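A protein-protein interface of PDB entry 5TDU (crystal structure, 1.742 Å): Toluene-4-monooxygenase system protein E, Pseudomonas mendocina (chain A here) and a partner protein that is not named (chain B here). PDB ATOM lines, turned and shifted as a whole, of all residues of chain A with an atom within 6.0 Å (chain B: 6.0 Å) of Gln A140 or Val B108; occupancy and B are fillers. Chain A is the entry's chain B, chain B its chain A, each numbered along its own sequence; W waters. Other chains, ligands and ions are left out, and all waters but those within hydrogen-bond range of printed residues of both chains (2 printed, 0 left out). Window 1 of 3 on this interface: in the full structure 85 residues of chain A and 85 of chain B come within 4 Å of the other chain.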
ATOM      1  N   HIS A  33     -12.318 -24.863   3.954  1.00  0.00           N
ATOM      2  CA  HIS A  33     -11.903 -26.207   4.402  1.00  0.00           C
ATOM      3  C   HIS A  33     -13.109 -27.062   4.785  1.00  0.00           C
ATOM      4  O   HIS A  33     -13.599 -26.961   5.911  1.00  0.00           O
ATOM      5  CB  HIS A  33     -10.983 -26.154   5.624  1.00  0.00           C
ATOM      6  CG  HIS A  33      -9.590 -25.686   5.347  1.00  0.00           C
ATOM      7  ND1 HIS A  33      -9.014 -25.720   4.095  1.00  0.00           N
ATOM      8  CD2 HIS A  33      -8.649 -25.186   6.184  1.00  0.00           C
ATOM      9  CE1 HIS A  33      -7.779 -25.252   4.171  1.00  0.00           C
ATOM     10  NE2 HIS A  33      -7.533 -24.923   5.430  1.00  0.00           N
ATOM     11  N   ARG A  59      -4.389 -32.095  13.623  1.00  0.00           N
ATOM     12  CA  ARG A  59      -5.222 -30.896  13.590  1.00  0.00           C
ATOM     13  C   ARG A  59      -6.304 -30.961  14.673  1.00  0.00           C
ATOM     14  O   ARG A  59      -6.295 -30.157  15.598  1.00  0.00           O
ATOM     15  CB  ARG A  59      -5.877 -30.687  12.225  1.00  0.00           C
ATOM     16  CG  ARG A  59      -6.837 -29.487  12.205  1.00  0.00           C
ATOM     17  CD  ARG A  59      -7.778 -29.538  11.020  1.00  0.00           C
ATOM     18  NE  ARG A  59      -7.212 -28.908   9.827  1.00  0.00           N
ATOM     19  CZ  ARG A  59      -7.646 -29.129   8.588  1.00  0.00           C
ATOM     20  NH1 ARG A  59      -8.649 -29.983   8.378  1.00  0.00           N
ATOM     21  NH2 ARG A  59      -7.071 -28.499   7.560  1.00  0.00           N
ATOM     22  N   SER A 135       8.295 -25.382   5.960  1.00  0.00           N
ATOM     23  CA  SER A 135       7.537 -25.342   7.202  1.00  0.00           C
ATOM     24  C   SER A 135       6.231 -24.570   7.006  1.00  0.00           C
ATOM     25  O   SER A 135       5.184 -24.974   7.519  1.00  0.00           O
ATOM     26  CB  SER A 135       8.388 -24.727   8.325  1.00  0.00           C
ATOM     27  OG  SER A 135       7.706 -24.771   9.571  1.00  0.00           O
ATOM     28  N   SER A 136       6.288 -23.474   6.245  1.00  0.00           N
ATOM     29  CA  SER A 136       5.089 -22.676   5.986  1.00  0.00           C
ATOM     30  C   SER A 136       4.053 -23.507   5.220  1.00  0.00           C
ATOM     31  O   SER A 136       2.846 -23.385   5.453  1.00  0.00           O
ATOM     32  CB  SER A 136       5.429 -21.403   5.193  1.00  0.00           C
ATOM     33  OG  SER A 136       6.284 -20.534   5.918  1.00  0.00           O
ATOM     34  N   ALA A 137       4.529 -24.333   4.287  1.00  0.00           N
ATOM     35  CA  ALA A 137       3.630 -25.193   3.519  1.00  0.00           C
ATOM     36  C   ALA A 137       2.974 -26.203   4.453  1.00  0.00           C
ATOM     37  O   ALA A 137       1.824 -26.590   4.249  1.00  0.00           O
ATOM     38  CB  ALA A 137       4.384 -25.922   2.377  1.00  0.00           C
ATOM     39  N   TYR A 138       3.694 -26.646   5.475  1.00  0.00           N
ATOM     40  CA  TYR A 138       3.073 -27.596   6.395  1.00  0.00           C
ATOM     41  C   TYR A 138       1.965 -26.916   7.216  1.00  0.00           C
ATOM     42  O   TYR A 138       0.872 -27.479   7.378  1.00  0.00           O
ATOM     43  CB  TYR A 138       4.101 -28.248   7.318  1.00  0.00           C
ATOM     44  CG  TYR A 138       3.440 -29.299   8.190  1.00  0.00           C
ATOM     45  CD1 TYR A 138       3.156 -29.042   9.525  1.00  0.00           C
ATOM     46  CD2 TYR A 138       3.052 -30.523   7.658  1.00  0.00           C
ATOM     47  CE1 TYR A 138       2.527 -29.997  10.313  1.00  0.00           C
ATOM     48  CE2 TYR A 138       2.418 -31.474   8.425  1.00  0.00           C
ATOM     49  CZ  TYR A 138       2.161 -31.209   9.758  1.00  0.00           C
ATOM     50  OH  TYR A 138       1.525 -32.150  10.537  1.00  0.00           O
ATOM     51  N   VAL A 139       2.216 -25.712   7.726  1.00  0.00           N
ATOM     52  CA  VAL A 139       1.159 -25.023   8.467  1.00  0.00           C
ATOM     53  C   VAL A 139      -0.038 -24.817   7.541  1.00  0.00           C
ATOM     54  O   VAL A 139      -1.188 -24.972   7.962  1.00  0.00           O
ATOM     55  CB  VAL A 139       1.638 -23.686   9.069  1.00  0.00           C
ATOM     56  CG1 VAL A 139       0.551 -23.081   9.983  1.00  0.00           C
ATOM     57  CG2 VAL A 139       2.920 -23.882   9.840  1.00  0.00           C
ATOM     58  N   GLN A 140       0.223 -24.468   6.282  1.00  0.00           N
ATOM     59  CA  GLN A 140      -0.857 -24.337   5.305  1.00  0.00           C
ATOM     60  C   GLN A 140      -1.769 -25.561   5.267  1.00  0.00           C
ATOM     61  O   GLN A 140      -2.999 -25.442   5.303  1.00  0.00           O
ATOM     62  CB  GLN A 140      -0.301 -24.110   3.889  1.00  0.00           C
ATOM     63  CG  GLN A 140      -1.365 -24.169   2.773  1.00  0.00           C
ATOM     64  CD  GLN A 140      -1.662 -25.582   2.272  1.00  0.00           C
ATOM     65  OE1 GLN A 140      -0.746 -26.373   1.993  1.00  0.00           O
ATOM     66  NE2 GLN A 140      -2.952 -25.904   2.150  1.00  0.00           N
ATOM     67  N   GLN A 141      -1.168 -26.733   5.115  1.00  0.00           N
ATOM     68  CA  GLN A 141      -1.969 -27.914   4.834  1.00  0.00           C
ATOM     69  C   GLN A 141      -2.674 -28.423   6.087  1.00  0.00           C
ATOM     70  O   GLN A 141      -3.663 -29.141   5.982  1.00  0.00           O
ATOM     71  CB  GLN A 141      -1.112 -29.020   4.197  1.00  0.00           C
ATOM     72  CG  GLN A 141      -0.006 -29.570   5.080  1.00  0.00           C
ATOM     73  CD  GLN A 141       1.097 -30.219   4.252  1.00  0.00           C
ATOM     74  OE1 GLN A 141       1.220 -31.448   4.193  1.00  0.00           O
ATOM     75  NE2 GLN A 141       1.894 -29.388   3.592  1.00  0.00           N
ATOM     76  N   MET A 142      -2.196 -28.012   7.262  1.00  0.00           N
ATOM     77  CA  MET A 142      -2.781 -28.466   8.533  1.00  0.00           C
ATOM     78  C   MET A 142      -3.697 -27.462   9.251  1.00  0.00           C
ATOM     79  O   MET A 142      -4.436 -27.851  10.152  1.00  0.00           O
ATOM     80  CB  MET A 142      -1.670 -28.873   9.515  1.00  0.00           C
ATOM     81  CG  MET A 142      -0.750 -29.985   9.020  1.00  0.00           C
ATOM     82  SD  MET A 142      -1.618 -31.448   8.416  1.00  0.00           S
ATOM     83  CE  MET A 142      -2.667 -31.844   9.820  1.00  0.00           C
ATOM     84  N   ALA A 143      -3.647 -26.184   8.892  1.00  0.00           N
ATOM     85  CA  ALA A 143      -4.415 -25.175   9.633  1.00  0.00           C
ATOM     86  C   ALA A 143      -5.918 -25.398   9.504  1.00  0.00           C
ATOM     87  O   ALA A 143      -6.406 -25.806   8.455  1.00  0.00           O
ATOM     88  CB  ALA A 143      -4.055 -23.779   9.166  1.00  0.00           C
ATOM     89  N   ILE A 148      -6.626 -18.881   7.598  1.00  0.00           N
ATOM     90  CA  ILE A 148      -5.300 -19.120   8.154  1.00  0.00           C
ATOM     91  C   ILE A 148      -4.381 -19.691   7.072  1.00  0.00           C
ATOM     92  O   ILE A 148      -3.258 -19.219   6.864  1.00  0.00           O
ATOM     93  CB  ILE A 148      -5.351 -20.078   9.371  1.00  0.00           C
ATOM     94  CG1 ILE A 148      -6.189 -19.473  10.492  1.00  0.00           C
ATOM     95  CG2 ILE A 148      -3.941 -20.363   9.871  1.00  0.00           C
ATOM     96  CD1 ILE A 148      -6.467 -20.463  11.649  1.00  0.00           C
ATOM     97  N   SER A 149      -4.857 -20.732   6.405  1.00  0.00           N
ATOM     98  CA  SER A 149      -4.055 -21.405   5.385  1.00  0.00           C
ATOM     99  C   SER A 149      -3.609 -20.428   4.295  1.00  0.00           C
ATOM    100  O   SER A 149      -2.489 -20.526   3.792  1.00  0.00           O
ATOM    101  CB  SER A 149      -4.836 -22.558   4.767  1.00  0.00           C
ATOM    102  OG  SER A 149      -4.995 -23.610   5.708  1.00  0.00           O
ATOM    103  N   ASN A 150      -4.474 -19.486   3.936  1.00  0.00           N
ATOM    104  CA  ASN A 150      -4.134 -18.533   2.869  1.00  0.00           C
ATOM    105  C   ASN A 150      -2.953 -17.650   3.274  1.00  0.00           C
ATOM    106  O   ASN A 150      -2.062 -17.387   2.457  1.00  0.00           O
ATOM    107  CB  ASN A 150      -5.346 -17.675   2.498  1.00  0.00           C
ATOM    108  CG  ASN A 150      -6.347 -18.431   1.645  1.00  0.00           C
ATOM    109  OD1 ASN A 150      -6.234 -19.655   1.469  1.00  0.00           O
ATOM    110  ND2 ASN A 150      -7.336 -17.717   1.114  1.00  0.00           N
ATOM    111  N   CYS A 152      -0.648 -18.610   5.137  1.00  0.00           N
ATOM    112  CA  CYS A 152       0.473 -19.544   5.052  1.00  0.00           C
ATOM    113  C   CYS A 152       0.929 -19.766   3.614  1.00  0.00           C
ATOM    114  O   CYS A 152       2.123 -19.905   3.370  1.00  0.00           O
ATOM    115  CB  CYS A 152       0.110 -20.892   5.687  1.00  0.00           C
ATOM    116  SG  CYS A 152      -0.107 -20.780   7.475  1.00  0.00           S
ATOM    117  N   ILE A 153      -0.010 -19.820   2.671  1.00  0.00           N
ATOM    118  CA  ILE A 153       0.365 -19.978   1.260  1.00  0.00           C
ATOM    119  C   ILE A 153       1.239 -18.807   0.834  1.00  0.00           C
ATOM    120  O   ILE A 153       2.304 -18.983   0.245  1.00  0.00           O
ATOM    121  CB  ILE A 153      -0.867 -20.063   0.329  1.00  0.00           C
ATOM    122  CG1 ILE A 153      -1.772 -21.249   0.701  1.00  0.00           C
ATOM    123  CG2 ILE A 153      -0.417 -20.085  -1.182  1.00  0.00           C
ATOM    124  CD1 ILE A 153      -3.197 -21.164   0.051  1.00  0.00           C
ATOM    125  N   THR A 156       4.608 -19.016   2.300  1.00  0.00           N
ATOM    126  CA  THR A 156       5.422 -20.020   1.628  1.00  0.00           C
ATOM    127  C   THR A 156       6.053 -19.387   0.383  1.00  0.00           C
ATOM    128  O   THR A 156       7.250 -19.544   0.120  1.00  0.00           O
ATOM    129  CB  THR A 156       4.587 -21.261   1.199  1.00  0.00           C
ATOM    130  OG1 THR A 156       3.885 -21.799   2.328  1.00  0.00           O
ATOM    131  CG2 THR A 156       5.486 -22.343   0.597  1.00  0.00           C
ATOM    132  N   GLY B 103     -12.864 -27.614  -4.868  1.00  0.00           N
ATOM    133  CA  GLY B 103     -11.906 -28.677  -5.166  1.00  0.00           C
ATOM    134  C   GLY B 103     -10.563 -28.106  -5.614  1.00  0.00           C
ATOM    135  O   GLY B 103      -9.491 -28.631  -5.273  1.00  0.00           O
ATOM    136  N   GLU B 104     -10.611 -27.029  -6.395  1.00  0.00           N
ATOM    137  CA  GLU B 104      -9.384 -26.296  -6.739  1.00  0.00           C
ATOM    138  C   GLU B 104      -8.667 -25.860  -5.468  1.00  0.00           C
ATOM    139  O   GLU B 104      -7.446 -25.979  -5.341  1.00  0.00           O
ATOM    140  CB  GLU B 104      -9.695 -25.064  -7.589  1.00  0.00           C
ATOM    141  CG  GLU B 104     -10.309 -25.363  -8.937  1.00  0.00           C
ATOM    142  CD  GLU B 104      -9.278 -25.410 -10.046  1.00  0.00           C
ATOM    143  OE1 GLU B 104      -9.658 -25.189 -11.210  1.00  0.00           O
ATOM    144  OE2 GLU B 104      -8.092 -25.665  -9.747  1.00  0.00           O
ATOM    145  N   TYR B 105      -9.425 -25.304  -4.533  1.00  0.00           N
ATOM    146  CA  TYR B 105      -8.817 -24.849  -3.293  1.00  0.00           C
ATOM    147  C   TYR B 105      -8.240 -26.044  -2.533  1.00  0.00           C
ATOM    148  O   TYR B 105      -7.191 -25.934  -1.892  1.00  0.00           O
ATOM    149  CB  TYR B 105      -9.821 -24.080  -2.416  1.00  0.00           C
ATOM    150  CG  TYR B 105      -9.131 -23.497  -1.210  1.00  0.00           C
ATOM    151  CD1 TYR B 105      -8.278 -22.404  -1.344  1.00  0.00           C
ATOM    152  CD2 TYR B 105      -9.285 -24.064   0.055  1.00  0.00           C
ATOM    153  CE1 TYR B 105      -7.614 -21.886  -0.257  1.00  0.00           C
ATOM    154  CE2 TYR B 105      -8.627 -23.547   1.146  1.00  0.00           C
ATOM    155  CZ  TYR B 105      -7.789 -22.460   0.984  1.00  0.00           C
ATOM    156  OH  TYR B 105      -7.117 -21.949   2.069  1.00  0.00           O
ATOM    157  N   ALA B 106      -8.908 -27.193  -2.614  1.00  0.00           N
ATOM    158  CA  ALA B 106      -8.371 -28.404  -1.990  1.00  0.00           C
ATOM    159  C   ALA B 106      -7.054 -28.802  -2.656  1.00  0.00           C
ATOM    160  O   ALA B 106      -6.164 -29.346  -2.012  1.00  0.00           O
ATOM    161  CB  ALA B 106      -9.378 -29.555  -2.059  1.00  0.00           C
ATOM    162  N   ALA B 107      -6.907 -28.500  -3.942  1.00  0.00           N
ATOM    163  CA  ALA B 107      -5.681 -28.878  -4.636  1.00  0.00           C
ATOM    164  C   ALA B 107      -4.466 -28.119  -4.087  1.00  0.00           C
ATOM    165  O   ALA B 107      -3.329 -28.574  -4.250  1.00  0.00           O
ATOM    166  CB  ALA B 107      -5.826 -28.655  -6.144  1.00  0.00           C
ATOM    167  N   VAL B 108      -4.693 -26.976  -3.432  1.00  0.00           N
ATOM    168  CA  VAL B 108      -3.602 -26.273  -2.756  1.00  0.00           C
ATOM    169  C   VAL B 108      -2.895 -27.242  -1.811  1.00  0.00           C
ATOM    170  O   VAL B 108      -1.668 -27.250  -1.693  1.00  0.00           O
ATOM    171  CB  VAL B 108      -4.084 -25.048  -1.958  1.00  0.00           C
ATOM    172  CG1 VAL B 108      -2.916 -24.463  -1.158  1.00  0.00           C
ATOM    173  CG2 VAL B 108      -4.702 -23.984  -2.871  1.00  0.00           C
ATOM    174  N   THR B 109      -3.694 -28.055  -1.129  1.00  0.00           N
ATOM    175  CA  THR B 109      -3.183 -28.972  -0.118  1.00  0.00           C
ATOM    176  C   THR B 109      -2.371 -30.125  -0.737  1.00  0.00           C
ATOM    177  O   THR B 109      -1.366 -30.546  -0.171  1.00  0.00           O
ATOM    178  CB  THR B 109      -4.345 -29.506   0.742  1.00  0.00           C
ATOM    179  OG1 THR B 109      -4.777 -28.464   1.642  1.00  0.00           O
ATOM    180  CG2 THR B 109      -3.920 -30.731   1.555  1.00  0.00           C
ATOM    181  N   GLY B 110      -2.783 -30.623  -1.900  1.00  0.00           N
ATOM    182  CA  GLY B 110      -1.972 -31.600  -2.616  1.00  0.00           C
ATOM    183  C   GLY B 110      -0.611 -31.031  -2.985  1.00  0.00           C
ATOM    184  O   GLY B 110       0.441 -31.676  -2.831  1.00  0.00           O
ATOM    185  N   GLU B 111      -0.627 -29.805  -3.483  1.00  0.00           N
ATOM    186  CA  GLU B 111       0.607 -29.112  -3.828  1.00  0.00           C
ATOM    187  C   GLU B 111       1.423 -28.865  -2.554  1.00  0.00           C
ATOM    188  O   GLU B 111       2.637 -29.056  -2.539  1.00  0.00           O
ATOM    189  CB  GLU B 111       0.296 -27.804  -4.555  1.00  0.00           C
ATOM    190  CG  GLU B 111      -0.308 -27.999  -5.965  1.00  0.00           C
ATOM    191  CD  GLU B 111       0.701 -28.478  -7.007  1.00  0.00           C
ATOM    192  OE1 GLU B 111       1.909 -28.453  -6.716  1.00  0.00           O
ATOM    193  OE2 GLU B 111       0.290 -28.864  -8.133  1.00  0.00           O
ATOM    194  N   GLY B 112       0.751 -28.465  -1.478  1.00  0.00           N
ATOM    195  CA  GLY B 112       1.428 -28.260  -0.209  1.00  0.00           C
ATOM    196  C   GLY B 112       2.090 -29.515   0.335  1.00  0.00           C
ATOM    197  O   GLY B 112       3.176 -29.458   0.913  1.00  0.00           O
ATOM    198  N   ARG B 113       1.429 -30.651   0.145  1.00  0.00           N
ATOM    199  CA  ARG B 113       1.958 -31.937   0.591  1.00  0.00           C
ATOM    200  C   ARG B 113       3.312 -32.182  -0.082  1.00  0.00           C
ATOM    201  O   ARG B 113       4.248 -32.659   0.549  1.00  0.00           O
ATOM    202  CB  ARG B 113       0.977 -33.068   0.271  1.00  0.00           C
ATOM    203  CG  ARG B 113       1.227 -34.370   1.055  1.00  0.00           C
ATOM    204  CD  ARG B 113       0.540 -34.313   2.436  1.00  0.00           C
ATOM    205  NE  ARG B 113      -0.918 -34.271   2.331  1.00  0.00           N
ATOM    206  CZ  ARG B 113      -1.727 -33.631   3.177  1.00  0.00           C
ATOM    207  NH1 ARG B 113      -1.226 -32.939   4.206  1.00  0.00           N
ATOM    208  NH2 ARG B 113      -3.045 -33.675   2.991  1.00  0.00           N
ATOM    209  N   ALA B 127       6.019 -27.037  -6.613  1.00  0.00           N
ATOM    210  CA  ALA B 127       4.782 -27.234  -5.846  1.00  0.00           C
ATOM    211  C   ALA B 127       4.395 -25.963  -5.090  1.00  0.00           C
ATOM    212  O   ALA B 127       3.233 -25.751  -4.765  1.00  0.00           O
ATOM    213  CB  ALA B 127       4.930 -28.403  -4.869  1.00  0.00           C
ATOM    214  N   GLY B 130       2.696 -24.190  -7.550  1.00  0.00           N
ATOM    215  CA  GLY B 130       1.456 -24.951  -7.644  1.00  0.00           C
ATOM    216  C   GLY B 130       0.441 -24.577  -6.574  1.00  0.00           C
ATOM    217  O   GLY B 130      -0.754 -24.462  -6.858  1.00  0.00           O
ATOM    218  N   MET B 131       0.912 -24.385  -5.343  1.00  0.00           N
ATOM    219  CA  MET B 131       0.039 -23.928  -4.252  1.00  0.00           C
ATOM    220  C   MET B 131      -0.622 -22.622  -4.653  1.00  0.00           C
ATOM    221  O   MET B 131      -1.830 -22.416  -4.482  1.00  0.00           O
ATOM    222  CB  MET B 131       0.828 -23.723  -2.955  1.00  0.00           C
ATOM    223  CG  MET B 131       1.261 -25.028  -2.264  1.00  0.00           C
ATOM    224  SD  MET B 131       2.522 -24.748  -0.999  1.00  0.00           S
ATOM    225  CE  MET B 131       1.545 -23.931   0.266  1.00  0.00           C
ATOM    226  N   MET B 132       0.201 -21.724  -5.167  1.00  0.00           N
ATOM    227  CA  MET B 132      -0.262 -20.406  -5.576  1.00  0.00           C
ATOM    228  C   MET B 132      -1.239 -20.500  -6.742  1.00  0.00           C
ATOM    229  O   MET B 132      -2.271 -19.827  -6.735  1.00  0.00           O
ATOM    230  CB  MET B 132       0.936 -19.518  -5.917  1.00  0.00           C
ATOM    231  CG  MET B 132       1.741 -19.108  -4.689  1.00  0.00           C
ATOM    232  SD  MET B 132       0.907 -17.827  -3.726  1.00  0.00           S
ATOM    233  CE  MET B 132       1.165 -16.364  -4.773  1.00  0.00           C
ATOM    234  N   GLU B 134      -3.275 -22.972  -7.526  1.00  0.00           N
ATOM    235  CA  GLU B 134      -4.571 -23.528  -7.158  1.00  0.00           C
ATOM    236  C   GLU B 134      -5.336 -22.525  -6.294  1.00  0.00           C
ATOM    237  O   GLU B 134      -6.564 -22.486  -6.320  1.00  0.00           O
ATOM    238  CB  GLU B 134      -4.413 -24.867  -6.427  1.00  0.00           C
ATOM    239  CG  GLU B 134      -3.669 -25.955  -7.233  1.00  0.00           C
ATOM    240  CD  GLU B 134      -4.344 -26.346  -8.543  1.00  0.00           C
ATOM    241  OE1 GLU B 134      -5.284 -25.659  -9.007  1.00  0.00           O
ATOM    242  OE2 GLU B 134      -3.931 -27.370  -9.116  1.00  0.00           O
ATOM    243  N   LEU B 135      -4.612 -21.706  -5.536  1.00  0.00           N
ATOM    244  CA  LEU B 135      -5.253 -20.617  -4.805  1.00  0.00           C
ATOM    245  C   LEU B 135      -5.933 -19.678  -5.797  1.00  0.00           C
ATOM    246  O   LEU B 135      -7.100 -19.305  -5.630  1.00  0.00           O
ATOM    247  CB  LEU B 135      -4.233 -19.854  -3.946  1.00  0.00           C
ATOM    248  CG  LEU B 135      -4.774 -18.672  -3.136  1.00  0.00           C
ATOM    249  CD1 LEU B 135      -5.763 -19.171  -2.081  1.00  0.00           C
ATOM    250  CD2 LEU B 135      -3.629 -17.925  -2.479  1.00  0.00           C
ATOM    251  N   ILE B 180      -5.834 -36.213  -4.162  1.00  0.00           N
ATOM    252  CA  ILE B 180      -5.204 -34.922  -3.874  1.00  0.00           C
ATOM    253  C   ILE B 180      -4.785 -34.781  -2.418  1.00  0.00           C
ATOM    254  O   ILE B 180      -3.624 -34.518  -2.124  1.00  0.00           O
ATOM    255  CB  ILE B 180      -6.130 -33.749  -4.239  1.00  0.00           C
ATOM    256  CG1 ILE B 180      -6.515 -33.803  -5.715  1.00  0.00           C
ATOM    257  CG2 ILE B 180      -5.468 -32.407  -3.865  1.00  0.00           C
ATOM    258  CD1 ILE B 180      -7.246 -32.550  -6.187  1.00  0.00           C
HETATM  259  O   HOH W   1      -5.358 -24.309   1.971  1.00  0.00           O
HETATM  260  O   HOH W   2      -5.562 -29.272   4.107  1.00  0.00           O
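OH of Tyr B105 lies within hydrogen-bond range of OD1 of Asn A150.
NE2 of Gln A140 is in hydrogen-bond range of OG1 of Thr B109, 3.2 Å away.
The backbone carbonyl oxygen (O) of Gly B112 lies within hydrogen-bond range of the side-chain amide nitrogen (NE2) of Gln A141 (3.0 Å).
OE1 of Gln A141 lies within hydrogen-bond range of NH1 of Arg B113, 2.9 Å away.
NE2 of His A33 sits close to O of Ala A143 (3.3 Å).
NE2 of His A33 is in hydrogen-bond range of OG of Ser A149, at 2.9 Å.
O of Ala A137 sits close to OE1 of Gln A140, at 3.4 Å.
The backbone carbonyl oxygen of Ala A137 sits at hydrogen-bond distance from the side-chain amide nitrogen of Gln A141, at 2.9 Å.
O of Gln A140 sits at hydrogen-bond distance from OG of Ser A149 (2.7 Å).
O of Cys A152 is in hydrogen-bond range of OG1 of Thr A156, 2.8 Å away.
His A33 touches Tyr B105 (CE1 to CE2, 3.6 Å).
Gln A140 touches Val B108 (NE2 to CG1, 3.6 Å).
CA of Gly B112 touches OE1 of Gln A140, 3.6 Å away.
Gln A140 touches Met B131.
CB of Ser A149 touches OH of Tyr B105 (3.6 Å).
Asn A150 touches Leu B135 (OD1 to CD1, 3.6 Å).
Val B108 touches Ile A153 (CG1 to CD1, 3.5 Å).
CG2 of Ile A153 touches SD of Met B132 (3.7 Å).
Leu B135 touches Ile A153 (CD1 to CD1, 3.9 Å).
Met B131 touches Thr A156.
Of the printed residues of chain B, Gln A140 touches Val B108, Thr B109, Gly B112 and Met B131.
Of the printed residues of chain A, Arg B113 touches Gln A141 (2.9 Å).
Of the printed residues of chain B, Ser A149 touches Tyr B105.
Cys A152 touches none of the printed residues of chain B.
The nearest residue of chain B that does not touch Gln A140 is Arg B113 (5.1 Å).
The nearest printed residue of chain A that does not touch Met B131 is Ala A137 (4.03 Å).
Of the 17 printed residues of chain A, 7 touch a printed residue of chain B.
Printed residues of chain A that touch a printed residue of chain B: His A33, Gln A140, Gln A141, Ser A149, Asn A150, Ile A153 and Thr A156.
Hydrophobic or aromatic side chains of chain A that line the printed part of chain B: His A33 and Ile A153.
Printed residues of chain B that touch a printed residue of chain A: Tyr B105, Val B108, Thr B109, Gly B112, Arg B113, Met B131, Met B132 and Leu B135.
Hydrophobic or aromatic side chains of chain B that line the printed part of chain A: Tyr B105, Val B108, Met B131, Met B132 and Leu B135.
Among the printed residues, 14 pairs touch across the chains.
Among the printed residues, no Asp or Glu carboxylate lies within 4 Å of a Lys or Arg side-chain nitrogen of the other chain.
Water W2 lies within hydrogen-bond range of O of Gln A141 and OG1 of Thr B109.
Water W1 lies within hydrogen-bond range of the side-chain amide nitrogen (NE2) of Gln A140 (2.9 Å) and the side-chain hydroxyl (OH) of Tyr B105 (2.9 Å).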
